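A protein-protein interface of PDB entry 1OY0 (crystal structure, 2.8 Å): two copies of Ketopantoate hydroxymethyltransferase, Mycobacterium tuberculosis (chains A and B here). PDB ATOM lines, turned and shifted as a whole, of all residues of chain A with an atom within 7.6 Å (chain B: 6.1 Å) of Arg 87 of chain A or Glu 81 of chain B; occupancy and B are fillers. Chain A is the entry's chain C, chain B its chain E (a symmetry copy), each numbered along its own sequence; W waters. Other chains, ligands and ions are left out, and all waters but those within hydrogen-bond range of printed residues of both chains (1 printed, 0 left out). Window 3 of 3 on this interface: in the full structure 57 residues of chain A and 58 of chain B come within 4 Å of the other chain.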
ATOM      1  N   ASP A  43       9.896   2.369  25.511  1.00  0.00           N
ATOM      2  CA  ASP A  43       9.325   2.975  26.708  1.00  0.00           C
ATOM      3  C   ASP A  43       8.973   1.930  27.757  1.00  0.00           C
ATOM      4  O   ASP A  43       8.944   0.736  27.479  1.00  0.00           O
ATOM      5  CB  ASP A  43       8.094   3.833  26.380  1.00  0.00           C
ATOM      6  CG  ASP A  43       6.927   3.021  25.878  1.00  0.00           C
ATOM      7  OD1 ASP A  43       6.668   3.051  24.658  1.00  0.00           O
ATOM      8  OD2 ASP A  43       6.269   2.350  26.702  1.00  0.00           O
ATOM      9  N   TYR A  44       8.717   2.398  28.969  1.00  0.00           N
ATOM     10  CA  TYR A  44       8.394   1.532  30.090  1.00  0.00           C
ATOM     11  C   TYR A  44       7.201   0.597  29.893  1.00  0.00           C
ATOM     12  O   TYR A  44       7.302  -0.610  30.112  1.00  0.00           O
ATOM     13  CB  TYR A  44       8.153   2.386  31.328  1.00  0.00           C
ATOM     14  CG  TYR A  44       7.716   1.585  32.520  1.00  0.00           C
ATOM     15  CD1 TYR A  44       8.637   0.864  33.273  1.00  0.00           C
ATOM     16  CD2 TYR A  44       6.375   1.530  32.887  1.00  0.00           C
ATOM     17  CE1 TYR A  44       8.230   0.108  34.363  1.00  0.00           C
ATOM     18  CE2 TYR A  44       5.958   0.778  33.973  1.00  0.00           C
ATOM     19  CZ  TYR A  44       6.891   0.071  34.709  1.00  0.00           C
ATOM     20  OH  TYR A  44       6.491  -0.657  35.802  1.00  0.00           O
ATOM     21  N   VAL A  60      16.528  -1.114  22.305  1.00  0.00           N
ATOM     22  CA  VAL A  60      16.137   0.288  22.306  1.00  0.00           C
ATOM     23  C   VAL A  60      16.898   0.828  21.100  1.00  0.00           C
ATOM     24  O   VAL A  60      17.962   1.437  21.220  1.00  0.00           O
ATOM     25  CB  VAL A  60      16.586   1.016  23.580  1.00  0.00           C
ATOM     26  CG1 VAL A  60      15.952   2.386  23.635  1.00  0.00           C
ATOM     27  CG2 VAL A  60      16.205   0.214  24.799  1.00  0.00           C
ATOM     28  N   TYR A  69      10.365   9.865  17.571  1.00  0.00           N
ATOM     29  CA  TYR A  69      10.527  11.292  17.355  1.00  0.00           C
ATOM     30  C   TYR A  69      10.100  11.887  16.020  1.00  0.00           C
ATOM     31  O   TYR A  69      10.131  13.103  15.836  1.00  0.00           O
ATOM     32  CB  TYR A  69      11.971  11.661  17.658  1.00  0.00           C
ATOM     33  CG  TYR A  69      12.363  11.271  19.061  1.00  0.00           C
ATOM     34  CD1 TYR A  69      13.296  10.262  19.293  1.00  0.00           C
ATOM     35  CD2 TYR A  69      11.783  11.898  20.165  1.00  0.00           C
ATOM     36  CE1 TYR A  69      13.637   9.889  20.588  1.00  0.00           C
ATOM     37  CE2 TYR A  69      12.119  11.533  21.459  1.00  0.00           C
ATOM     38  CZ  TYR A  69      13.042  10.529  21.661  1.00  0.00           C
ATOM     39  OH  TYR A  69      13.354  10.158  22.938  1.00  0.00           O
ATOM     40  N   ASP A  80      21.199  11.666  23.962  1.00  0.00           N
ATOM     41  CA  ASP A  80      20.261  12.146  24.975  1.00  0.00           C
ATOM     42  C   ASP A  80      18.798  11.855  24.677  1.00  0.00           C
ATOM     43  O   ASP A  80      17.964  11.872  25.578  1.00  0.00           O
ATOM     44  CB  ASP A  80      20.472  13.637  25.244  1.00  0.00           C
ATOM     45  CG  ASP A  80      21.825  13.919  25.858  1.00  0.00           C
ATOM     46  OD1 ASP A  80      22.219  13.186  26.786  1.00  0.00           O
ATOM     47  OD2 ASP A  80      22.499  14.868  25.419  1.00  0.00           O
ATOM     48  N   LEU A  82      17.966   9.047  23.596  1.00  0.00           N
ATOM     49  CA  LEU A  82      17.889   7.615  23.804  1.00  0.00           C
ATOM     50  C   LEU A  82      18.060   7.170  25.255  1.00  0.00           C
ATOM     51  O   LEU A  82      17.238   6.410  25.768  1.00  0.00           O
ATOM     52  CB  LEU A  82      18.918   6.918  22.922  1.00  0.00           C
ATOM     53  CG  LEU A  82      18.563   6.892  21.432  1.00  0.00           C
ATOM     54  CD1 LEU A  82      19.794   6.560  20.597  1.00  0.00           C
ATOM     55  CD2 LEU A  82      17.453   5.879  21.191  1.00  0.00           C
ATOM     56  N   ILE A  83      19.110   7.641  25.921  1.00  0.00           N
ATOM     57  CA  ILE A  83      19.357   7.240  27.305  1.00  0.00           C
ATOM     58  C   ILE A  83      18.116   7.252  28.200  1.00  0.00           C
ATOM     59  O   ILE A  83      17.855   6.288  28.919  1.00  0.00           O
ATOM     60  CB  ILE A  83      20.473   8.104  27.952  1.00  0.00           C
ATOM     61  CG1 ILE A  83      21.809   7.797  27.273  1.00  0.00           C
ATOM     62  CG2 ILE A  83      20.576   7.818  29.444  1.00  0.00           C
ATOM     63  CD1 ILE A  83      22.999   8.502  27.898  1.00  0.00           C
ATOM     64  N   PRO A  84      17.340   8.344  28.182  1.00  0.00           N
ATOM     65  CA  PRO A  84      16.155   8.332  29.045  1.00  0.00           C
ATOM     66  C   PRO A  84      15.148   7.252  28.659  1.00  0.00           C
ATOM     67  O   PRO A  84      14.422   6.753  29.514  1.00  0.00           O
ATOM     68  CB  PRO A  84      15.609   9.758  28.917  1.00  0.00           C
ATOM     69  CG  PRO A  84      16.173  10.240  27.625  1.00  0.00           C
ATOM     70  CD  PRO A  84      17.543   9.670  27.579  1.00  0.00           C
ATOM     71  N   LEU A  85      15.112   6.888  27.377  1.00  0.00           N
ATOM     72  CA  LEU A  85      14.209   5.842  26.915  1.00  0.00           C
ATOM     73  C   LEU A  85      14.747   4.496  27.377  1.00  0.00           C
ATOM     74  O   LEU A  85      13.989   3.618  27.774  1.00  0.00           O
ATOM     75  CB  LEU A  85      14.095   5.839  25.392  1.00  0.00           C
ATOM     76  CG  LEU A  85      13.500   7.064  24.706  1.00  0.00           C
ATOM     77  CD1 LEU A  85      13.369   6.771  23.228  1.00  0.00           C
ATOM     78  CD2 LEU A  85      12.145   7.409  25.291  1.00  0.00           C
ATOM     79  N   VAL A  86      16.062   4.332  27.315  1.00  0.00           N
ATOM     80  CA  VAL A  86      16.690   3.095  27.753  1.00  0.00           C
ATOM     81  C   VAL A  86      16.341   2.856  29.212  1.00  0.00           C
ATOM     82  O   VAL A  86      15.904   1.769  29.581  1.00  0.00           O
ATOM     83  CB  VAL A  86      18.232   3.153  27.606  1.00  0.00           C
ATOM     84  CG1 VAL A  86      18.870   1.950  28.286  1.00  0.00           C
ATOM     85  CG2 VAL A  86      18.614   3.168  26.138  1.00  0.00           C
ATOM     86  N   ARG A  87      16.529   3.876  30.041  1.00  0.00           N
ATOM     87  CA  ARG A  87      16.221   3.750  31.456  1.00  0.00           C
ATOM     88  C   ARG A  87      14.798   3.239  31.635  1.00  0.00           C
ATOM     89  O   ARG A  87      14.546   2.355  32.459  1.00  0.00           O
ATOM     90  CB  ARG A  87      16.390   5.093  32.167  1.00  0.00           C
ATOM     91  CG  ARG A  87      17.822   5.605  32.193  1.00  0.00           C
ATOM     92  CD  ARG A  87      17.979   6.741  33.185  1.00  0.00           C
ATOM     93  NE  ARG A  87      17.187   7.907  32.818  1.00  0.00           N
ATOM     94  CZ  ARG A  87      17.710   9.056  32.412  1.00  0.00           C
ATOM     95  NH1 ARG A  87      19.024   9.183  32.328  1.00  0.00           N
ATOM     96  NH2 ARG A  87      16.924  10.070  32.078  1.00  0.00           N
ATOM     97  N   GLY A  88      13.868   3.785  30.855  1.00  0.00           N
ATOM     98  CA  GLY A  88      12.486   3.356  30.950  1.00  0.00           C
ATOM     99  C   GLY A  88      12.317   1.895  30.574  1.00  0.00           C
ATOM    100  O   GLY A  88      11.652   1.135  31.275  1.00  0.00           O
ATOM    101  N   VAL A  89      12.922   1.497  29.461  1.00  0.00           N
ATOM    102  CA  VAL A  89      12.827   0.121  29.009  1.00  0.00           C
ATOM    103  C   VAL A  89      13.471  -0.808  30.020  1.00  0.00           C
ATOM    104  O   VAL A  89      12.960  -1.894  30.299  1.00  0.00           O
ATOM    105  CB  VAL A  89      13.510  -0.067  27.648  1.00  0.00           C
ATOM    106  CG1 VAL A  89      13.639  -1.550  27.335  1.00  0.00           C
ATOM    107  CG2 VAL A  89      12.703   0.632  26.565  1.00  0.00           C
ATOM    108  N   VAL A  90      14.595  -0.381  30.576  1.00  0.00           N
ATOM    109  CA  VAL A  90      15.288  -1.197  31.558  1.00  0.00           C
ATOM    110  C   VAL A  90      14.393  -1.453  32.764  1.00  0.00           C
ATOM    111  O   VAL A  90      14.402  -2.540  33.329  1.00  0.00           O
ATOM    112  CB  VAL A  90      16.602  -0.523  32.005  1.00  0.00           C
ATOM    113  CG1 VAL A  90      17.193  -1.250  33.203  1.00  0.00           C
ATOM    114  CG2 VAL A  90      17.596  -0.525  30.849  1.00  0.00           C
ATOM    115  N   ARG A  91      13.611  -0.456  33.152  1.00  0.00           N
ATOM    116  CA  ARG A  91      12.715  -0.598  34.289  1.00  0.00           C
ATOM    117  C   ARG A  91      11.509  -1.473  33.973  1.00  0.00           C
ATOM    118  O   ARG A  91      10.977  -2.143  34.850  1.00  0.00           O
ATOM    119  CB  ARG A  91      12.237   0.779  34.746  1.00  0.00           C
ATOM    120  CG  ARG A  91      13.325   1.639  35.343  1.00  0.00           C
ATOM    121  CD  ARG A  91      12.912   3.100  35.430  1.00  0.00           C
ATOM    122  NE  ARG A  91      14.046   3.931  35.830  1.00  0.00           N
ATOM    123  CZ  ARG A  91      14.316   5.134  35.331  1.00  0.00           C
ATOM    124  NH1 ARG A  91      13.533   5.668  34.405  1.00  0.00           N
ATOM    125  NH2 ARG A  91      15.378   5.801  35.751  1.00  0.00           N
ATOM    126  N   GLY A  92      11.084  -1.476  32.717  1.00  0.00           N
ATOM    127  CA  GLY A  92       9.923  -2.261  32.340  1.00  0.00           C
ATOM    128  C   GLY A  92      10.144  -3.726  32.005  1.00  0.00           C
ATOM    129  O   GLY A  92       9.190  -4.506  32.014  1.00  0.00           O
ATOM    130  N   ALA A  93      11.384  -4.111  31.710  1.00  0.00           N
ATOM    131  CA  ALA A  93      11.681  -5.496  31.363  1.00  0.00           C
ATOM    132  C   ALA A  93      12.767  -6.071  32.256  1.00  0.00           C
ATOM    133  O   ALA A  93      13.916  -6.201  31.845  1.00  0.00           O
ATOM    134  CB  ALA A  93      12.101  -5.586  29.901  1.00  0.00           C
ATOM    135  N   VAL A  98      18.364  -6.133  27.866  1.00  0.00           N
ATOM    136  CA  VAL A  98      18.145  -4.870  27.183  1.00  0.00           C
ATOM    137  C   VAL A  98      19.393  -4.373  26.472  1.00  0.00           C
ATOM    138  O   VAL A  98      20.429  -4.151  27.093  1.00  0.00           O
ATOM    139  CB  VAL A  98      17.657  -3.801  28.173  1.00  0.00           C
ATOM    140  CG1 VAL A  98      17.419  -2.489  27.458  1.00  0.00           C
ATOM    141  CG2 VAL A  98      16.390  -4.277  28.845  1.00  0.00           C
ATOM    142  N   ARG A 120      28.056   5.354  28.881  1.00  0.00           N
ATOM    143  CA  ARG A 120      26.919   6.162  29.302  1.00  0.00           C
ATOM    144  C   ARG A 120      25.670   5.306  29.288  1.00  0.00           C
ATOM    145  O   ARG A 120      24.880   5.340  30.228  1.00  0.00           O
ATOM    146  CB  ARG A 120      26.720   7.365  28.380  1.00  0.00           C
ATOM    147  CG  ARG A 120      27.728   8.472  28.571  1.00  0.00           C
ATOM    148  CD  ARG A 120      27.292   9.723  27.843  1.00  0.00           C
ATOM    149  NE  ARG A 120      26.038  10.251  28.372  1.00  0.00           N
ATOM    150  CZ  ARG A 120      25.352  11.242  27.815  1.00  0.00           C
ATOM    151  NH1 ARG A 120      25.794  11.820  26.709  1.00  0.00           N
ATOM    152  NH2 ARG A 120      24.217  11.649  28.359  1.00  0.00           N
ATOM    153  N   PHE A 121      25.499   4.530  28.221  1.00  0.00           N
ATOM    154  CA  PHE A 121      24.337   3.661  28.097  1.00  0.00           C
ATOM    155  C   PHE A 121      24.251   2.605  29.187  1.00  0.00           C
ATOM    156  O   PHE A 121      23.152   2.179  29.546  1.00  0.00           O
ATOM    157  CB  PHE A 121      24.301   2.992  26.725  1.00  0.00           C
ATOM    158  CG  PHE A 121      23.817   3.893  25.639  1.00  0.00           C
ATOM    159  CD1 PHE A 121      24.712   4.533  24.796  1.00  0.00           C
ATOM    160  CD2 PHE A 121      22.459   4.132  25.481  1.00  0.00           C
ATOM    161  CE1 PHE A 121      24.258   5.404  23.805  1.00  0.00           C
ATOM    162  CE2 PHE A 121      21.991   4.993  24.504  1.00  0.00           C
ATOM    163  CZ  PHE A 121      22.892   5.631  23.663  1.00  0.00           C
ATOM    164  N   LYS A 123      26.154   2.727  32.500  1.00  0.00           N
ATOM    165  CA  LYS A 123      26.121   3.385  33.799  1.00  0.00           C
ATOM    166  C   LYS A 123      24.892   4.261  34.003  1.00  0.00           C
ATOM    167  O   LYS A 123      24.337   4.314  35.100  1.00  0.00           O
ATOM    168  CB  LYS A 123      27.375   4.239  34.000  1.00  0.00           C
ATOM    169  CG  LYS A 123      28.681   3.478  33.957  1.00  0.00           C
ATOM    170  CD  LYS A 123      29.844   4.372  34.335  1.00  0.00           C
ATOM    171  CE  LYS A 123      29.882   4.679  35.817  1.00  0.00           C
ATOM    172  NZ  LYS A 123      30.399   3.528  36.603  1.00  0.00           N
ATOM    173  N   ASP A 124      24.469   4.950  32.947  1.00  0.00           N
ATOM    174  CA  ASP A 124      23.318   5.835  33.024  1.00  0.00           C
ATOM    175  C   ASP A 124      22.047   5.147  32.553  1.00  0.00           C
ATOM    176  O   ASP A 124      21.089   5.027  33.304  1.00  0.00           O
ATOM    177  CB  ASP A 124      23.580   7.083  32.178  1.00  0.00           C
ATOM    178  CG  ASP A 124      22.556   8.177  32.405  1.00  0.00           C
ATOM    179  OD1 ASP A 124      21.533   7.929  33.076  1.00  0.00           O
ATOM    180  OD2 ASP A 124      22.781   9.293  31.898  1.00  0.00           O
ATOM    181  N   GLY A 125      22.053   4.699  31.304  1.00  0.00           N
ATOM    182  CA  GLY A 125      20.891   4.041  30.738  1.00  0.00           C
ATOM    183  C   GLY A 125      20.499   2.764  31.450  1.00  0.00           C
ATOM    184  O   GLY A 125      19.326   2.392  31.467  1.00  0.00           O
ATOM    185  N   GLY A 126      21.481   2.090  32.040  1.00  0.00           N
ATOM    186  CA  GLY A 126      21.199   0.854  32.742  1.00  0.00           C
ATOM    187  C   GLY A 126      21.103  -0.325  31.793  1.00  0.00           C
ATOM    188  O   GLY A 126      20.664  -1.403  32.183  1.00  0.00           O
ATOM    189  N   ALA A 127      21.509  -0.115  30.545  1.00  0.00           N
ATOM    190  CA  ALA A 127      21.474  -1.166  29.543  1.00  0.00           C
ATOM    191  C   ALA A 127      22.424  -2.295  29.935  1.00  0.00           C
ATOM    192  O   ALA A 127      23.313  -2.106  30.764  1.00  0.00           O
ATOM    193  CB  ALA A 127      21.866  -0.599  28.189  1.00  0.00           C
ATOM    194  N   ALA B  64       3.885  10.889  31.847  1.00  0.00           N
ATOM    195  CA  ALA B  64       4.831  10.107  31.063  1.00  0.00           C
ATOM    196  C   ALA B  64       5.857   9.503  32.019  1.00  0.00           C
ATOM    197  O   ALA B  64       6.472   8.476  31.735  1.00  0.00           O
ATOM    198  CB  ALA B  64       5.523  10.996  30.050  1.00  0.00           C
ATOM    199  N   TYR B  69       8.628   6.311  31.503  1.00  0.00           N
ATOM    200  CA  TYR B  69       9.882   6.025  32.178  1.00  0.00           C
ATOM    201  C   TYR B  69       9.870   5.091  33.368  1.00  0.00           C
ATOM    202  O   TYR B  69      10.925   4.750  33.887  1.00  0.00           O
ATOM    203  CB  TYR B  69      10.533   7.341  32.555  1.00  0.00           C
ATOM    204  CG  TYR B  69      10.740   8.210  31.352  1.00  0.00           C
ATOM    205  CD1 TYR B  69      10.013   9.386  31.181  1.00  0.00           C
ATOM    206  CD2 TYR B  69      11.664   7.853  30.369  1.00  0.00           C
ATOM    207  CE1 TYR B  69      10.205  10.191  30.055  1.00  0.00           C
ATOM    208  CE2 TYR B  69      11.865   8.648  29.242  1.00  0.00           C
ATOM    209  CZ  TYR B  69      11.133   9.813  29.094  1.00  0.00           C
ATOM    210  OH  TYR B  69      11.333  10.589  27.987  1.00  0.00           O
ATOM    211  N   TYR B  71       8.723   5.635  36.453  1.00  0.00           N
ATOM    212  CA  TYR B  71       8.876   6.248  37.764  1.00  0.00           C
ATOM    213  C   TYR B  71       7.558   5.974  38.468  1.00  0.00           C
ATOM    214  O   TYR B  71       6.505   5.944  37.832  1.00  0.00           O
ATOM    215  CB  TYR B  71       9.089   7.757  37.638  1.00  0.00           C
ATOM    216  CG  TYR B  71      10.402   8.153  37.008  1.00  0.00           C
ATOM    217  CD1 TYR B  71      10.441   8.972  35.872  1.00  0.00           C
ATOM    218  CD2 TYR B  71      11.610   7.719  37.545  1.00  0.00           C
ATOM    219  CE1 TYR B  71      11.658   9.344  35.288  1.00  0.00           C
ATOM    220  CE2 TYR B  71      12.824   8.084  36.972  1.00  0.00           C
ATOM    221  CZ  TYR B  71      12.843   8.893  35.841  1.00  0.00           C
ATOM    222  OH  TYR B  71      14.041   9.213  35.254  1.00  0.00           O
ATOM    223  N   PRO B  76      10.113  12.894  39.880  1.00  0.00           N
ATOM    224  CA  PRO B  76      11.432  12.827  39.253  1.00  0.00           C
ATOM    225  C   PRO B  76      11.591  13.260  37.798  1.00  0.00           C
ATOM    226  O   PRO B  76      12.655  13.731  37.418  1.00  0.00           O
ATOM    227  CB  PRO B  76      11.823  11.365  39.463  1.00  0.00           C
ATOM    228  CG  PRO B  76      10.519  10.667  39.363  1.00  0.00           C
ATOM    229  CD  PRO B  76       9.622  11.541  40.192  1.00  0.00           C
ATOM    230  N   ILE B  77      10.552  13.119  36.985  1.00  0.00           N
ATOM    231  CA  ILE B  77      10.679  13.470  35.573  1.00  0.00           C
ATOM    232  C   ILE B  77      11.196  14.884  35.341  1.00  0.00           C
ATOM    233  O   ILE B  77      10.746  15.836  35.975  1.00  0.00           O
ATOM    234  CB  ILE B  77       9.349  13.260  34.814  1.00  0.00           C
ATOM    235  CG1 ILE B  77       9.608  13.338  33.307  1.00  0.00           C
ATOM    236  CG2 ILE B  77       8.322  14.270  35.259  1.00  0.00           C
ATOM    237  CD1 ILE B  77       8.443  12.878  32.446  1.00  0.00           C
ATOM    238  N   SER B  78      12.154  15.006  34.425  1.00  0.00           N
ATOM    239  CA  SER B  78      12.767  16.291  34.110  1.00  0.00           C
ATOM    240  C   SER B  78      12.321  16.882  32.778  1.00  0.00           C
ATOM    241  O   SER B  78      11.783  16.189  31.920  1.00  0.00           O
ATOM    242  CB  SER B  78      14.283  16.145  34.069  1.00  0.00           C
ATOM    243  OG  SER B  78      14.684  15.586  32.836  1.00  0.00           O
ATOM    244  N   ILE B  79      12.567  18.174  32.610  1.00  0.00           N
ATOM    245  CA  ILE B  79      12.212  18.846  31.381  1.00  0.00           C
ATOM    246  C   ILE B  79      12.852  18.123  30.214  1.00  0.00           C
ATOM    247  O   ILE B  79      12.226  17.945  29.178  1.00  0.00           O
ATOM    248  CB  ILE B  79      12.699  20.305  31.362  1.00  0.00           C
ATOM    249  CG1 ILE B  79      11.867  21.136  32.325  1.00  0.00           C
ATOM    250  CG2 ILE B  79      12.572  20.883  29.971  1.00  0.00           C
ATOM    251  CD1 ILE B  79      12.236  22.602  32.341  1.00  0.00           C
ATOM    252  N   ASP B  80      14.098  17.701  30.379  1.00  0.00           N
ATOM    253  CA  ASP B  80      14.787  17.025  29.288  1.00  0.00           C
ATOM    254  C   ASP B  80      14.217  15.659  28.927  1.00  0.00           C
ATOM    255  O   ASP B  80      14.449  15.155  27.828  1.00  0.00           O
ATOM    256  CB  ASP B  80      16.284  16.930  29.583  1.00  0.00           C
ATOM    257  CG  ASP B  80      16.954  18.291  29.607  1.00  0.00           C
ATOM    258  OD1 ASP B  80      16.677  19.101  28.701  1.00  0.00           O
ATOM    259  OD2 ASP B  80      17.756  18.553  30.526  1.00  0.00           O
ATOM    260  N   GLU B  81      13.463  15.063  29.839  1.00  0.00           N
ATOM    261  CA  GLU B  81      12.850  13.779  29.555  1.00  0.00           C
ATOM    262  C   GLU B  81      11.523  14.018  28.851  1.00  0.00           C
ATOM    263  O   GLU B  81      10.867  13.078  28.417  1.00  0.00           O
ATOM    264  CB  GLU B  81      12.610  12.997  30.842  1.00  0.00           C
ATOM    265  CG  GLU B  81      13.864  12.471  31.481  1.00  0.00           C
ATOM    266  CD  GLU B  81      13.585  11.701  32.743  1.00  0.00           C
ATOM    267  OE1 GLU B  81      13.048  12.309  33.691  1.00  0.00           O
ATOM    268  OE2 GLU B  81      13.898  10.492  32.786  1.00  0.00           O
ATOM    269  N   LEU B  82      11.137  15.283  28.730  1.00  0.00           N
ATOM    270  CA  LEU B  82       9.879  15.631  28.087  1.00  0.00           C
ATOM    271  C   LEU B  82      10.017  16.338  26.743  1.00  0.00           C
ATOM    272  O   LEU B  82       9.383  15.941  25.774  1.00  0.00           O
ATOM    273  CB  LEU B  82       9.035  16.480  29.032  1.00  0.00           C
ATOM    274  CG  LEU B  82       8.416  15.729  30.211  1.00  0.00           C
ATOM    275  CD1 LEU B  82       7.979  16.704  31.291  1.00  0.00           C
ATOM    276  CD2 LEU B  82       7.234  14.914  29.722  1.00  0.00           C
ATOM    277  N   ILE B  83      10.839  17.377  26.674  1.00  0.00           N
ATOM    278  CA  ILE B  83      11.012  18.116  25.428  1.00  0.00           C
ATOM    279  C   ILE B  83      11.196  17.225  24.193  1.00  0.00           C
ATOM    280  O   ILE B  83      10.540  17.427  23.170  1.00  0.00           O
ATOM    281  CB  ILE B  83      12.194  19.115  25.524  1.00  0.00           C
ATOM    282  CG1 ILE B  83      11.850  20.224  26.523  1.00  0.00           C
ATOM    283  CG2 ILE B  83      12.488  19.721  24.160  1.00  0.00           C
ATOM    284  CD1 ILE B  83      12.918  21.324  26.635  1.00  0.00           C
ATOM    285  N   PRO B  84      12.099  16.237  24.256  1.00  0.00           N
ATOM    286  CA  PRO B  84      12.247  15.404  23.063  1.00  0.00           C
ATOM    287  C   PRO B  84      10.977  14.634  22.713  1.00  0.00           C
ATOM    288  O   PRO B  84      10.735  14.342  21.547  1.00  0.00           O
ATOM    289  CB  PRO B  84      13.437  14.508  23.402  1.00  0.00           C
ATOM    290  CG  PRO B  84      13.478  14.520  24.884  1.00  0.00           C
ATOM    291  CD  PRO B  84      13.129  15.915  25.255  1.00  0.00           C
ATOM    292  N   LEU B  85      10.165  14.314  23.716  1.00  0.00           N
ATOM    293  CA  LEU B  85       8.910  13.609  23.466  1.00  0.00           C
ATOM    294  C   LEU B  85       7.906  14.578  22.842  1.00  0.00           C
ATOM    295  O   LEU B  85       7.137  14.208  21.947  1.00  0.00           O
ATOM    296  CB  LEU B  85       8.316  13.049  24.761  1.00  0.00           C
ATOM    297  CG  LEU B  85       9.093  11.979  25.524  1.00  0.00           C
ATOM    298  CD1 LEU B  85       8.241  11.491  26.674  1.00  0.00           C
ATOM    299  CD2 LEU B  85       9.448  10.825  24.614  1.00  0.00           C
HETATM  300  O   HOH W   1      17.307   8.386  35.887  1.00  0.00           O
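Printed residues of chain B within 4 Å of Tyr 44 of chain A: Tyr 69.
Of the printed residues of chain B, Pro 84 of chain A touches Tyr 69 (3.1 Å).
Of the printed residues of chain B, Gly 88 of chain A touches Tyr 69.
Of the printed residues of chain B, Arg 91 of chain A touches Tyr 69 and Tyr 71.
Of the printed residues of chain A, Tyr 71 of chain B touches Arg 91 (3.6 Å).
Glu 81 of chain B touches just one residue of chain A: Arg 87.
The nearest printed residue of chain B that does not touch Pro 84 of chain A is Glu 81 of chain B (4.1 Å).
C of Tyr 69 of chain B touches CB of Tyr 44 of chain A, at 3.8 Å.
Pro 84 of chain B touches Tyr 69 of chain A (O to CD2, 3.0 Å).
Pro 84 of chain A touches Tyr 69 of chain B.
CA of Gly 88 of chain A touches O of Tyr 69 of chain B, 3.6 Å away.
Arg 91 of chain A touches Tyr 71 of chain B.
NH2 of Arg 87 of chain A is in salt-bridge range of OE2 of Glu 81 of chain B (3.1 Å).
NH1 of Arg 91 of chain A sits at hydrogen-bond distance from O of Tyr 69 of chain B (2.8 Å).
The guanidinium group (NH1) of Arg 87 of chain A is in salt-bridge range of the side-chain carboxylate (OD1) of Asp 124 of chain A (2.9 Å).
The backbone NH (N) of Arg 87 of chain A lies close to the backbone carbonyl oxygen (O) of Gly 125 of chain A (3.5 Å).
O of Ala 64 of chain B is in hydrogen-bond range of N of Tyr 69 of chain B (3.1 Å).
The side-chain hydroxyl (OH) of Tyr 69 of chain B is in hydrogen-bond range of the backbone carbonyl oxygen (O) of Glu 81 of chain B (2.6 Å).
OH of Tyr 71 of chain B is in hydrogen-bond range of OE2 of Glu 81 of chain B (2.8 Å).
The side-chain carboxylate of Glu 81 of chain B lies within hydrogen-bond range of the backbone NH of Ser 78 of chain B (2.9 Å).
Water W1 lies within hydrogen-bond range of NE of Arg 87 of chain A (3.1 Å), NH2 of Arg 91 of chain A (3.2 Å) and OH of Tyr 71 of chain B (3.4 Å).
Tyr 69 of chain A touches Pro 84 of chain B, and with the chains exchanged Pro 84 of chain A touches Tyr 69 of chain B.
Positions printed for both chains: 69, 80, 82, 83, 84 and 85.
Printed residues of chain B that touch a printed residue of chain A: Tyr 69, Tyr 71, Glu 81 and Pro 84.
Among the printed residues, Asp or Glu carboxylates within 4 Å of a Lys or Arg side-chain nitrogen of the other chain: Arg 87 of chain A with Glu 81 of chain B (3.1 Å).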
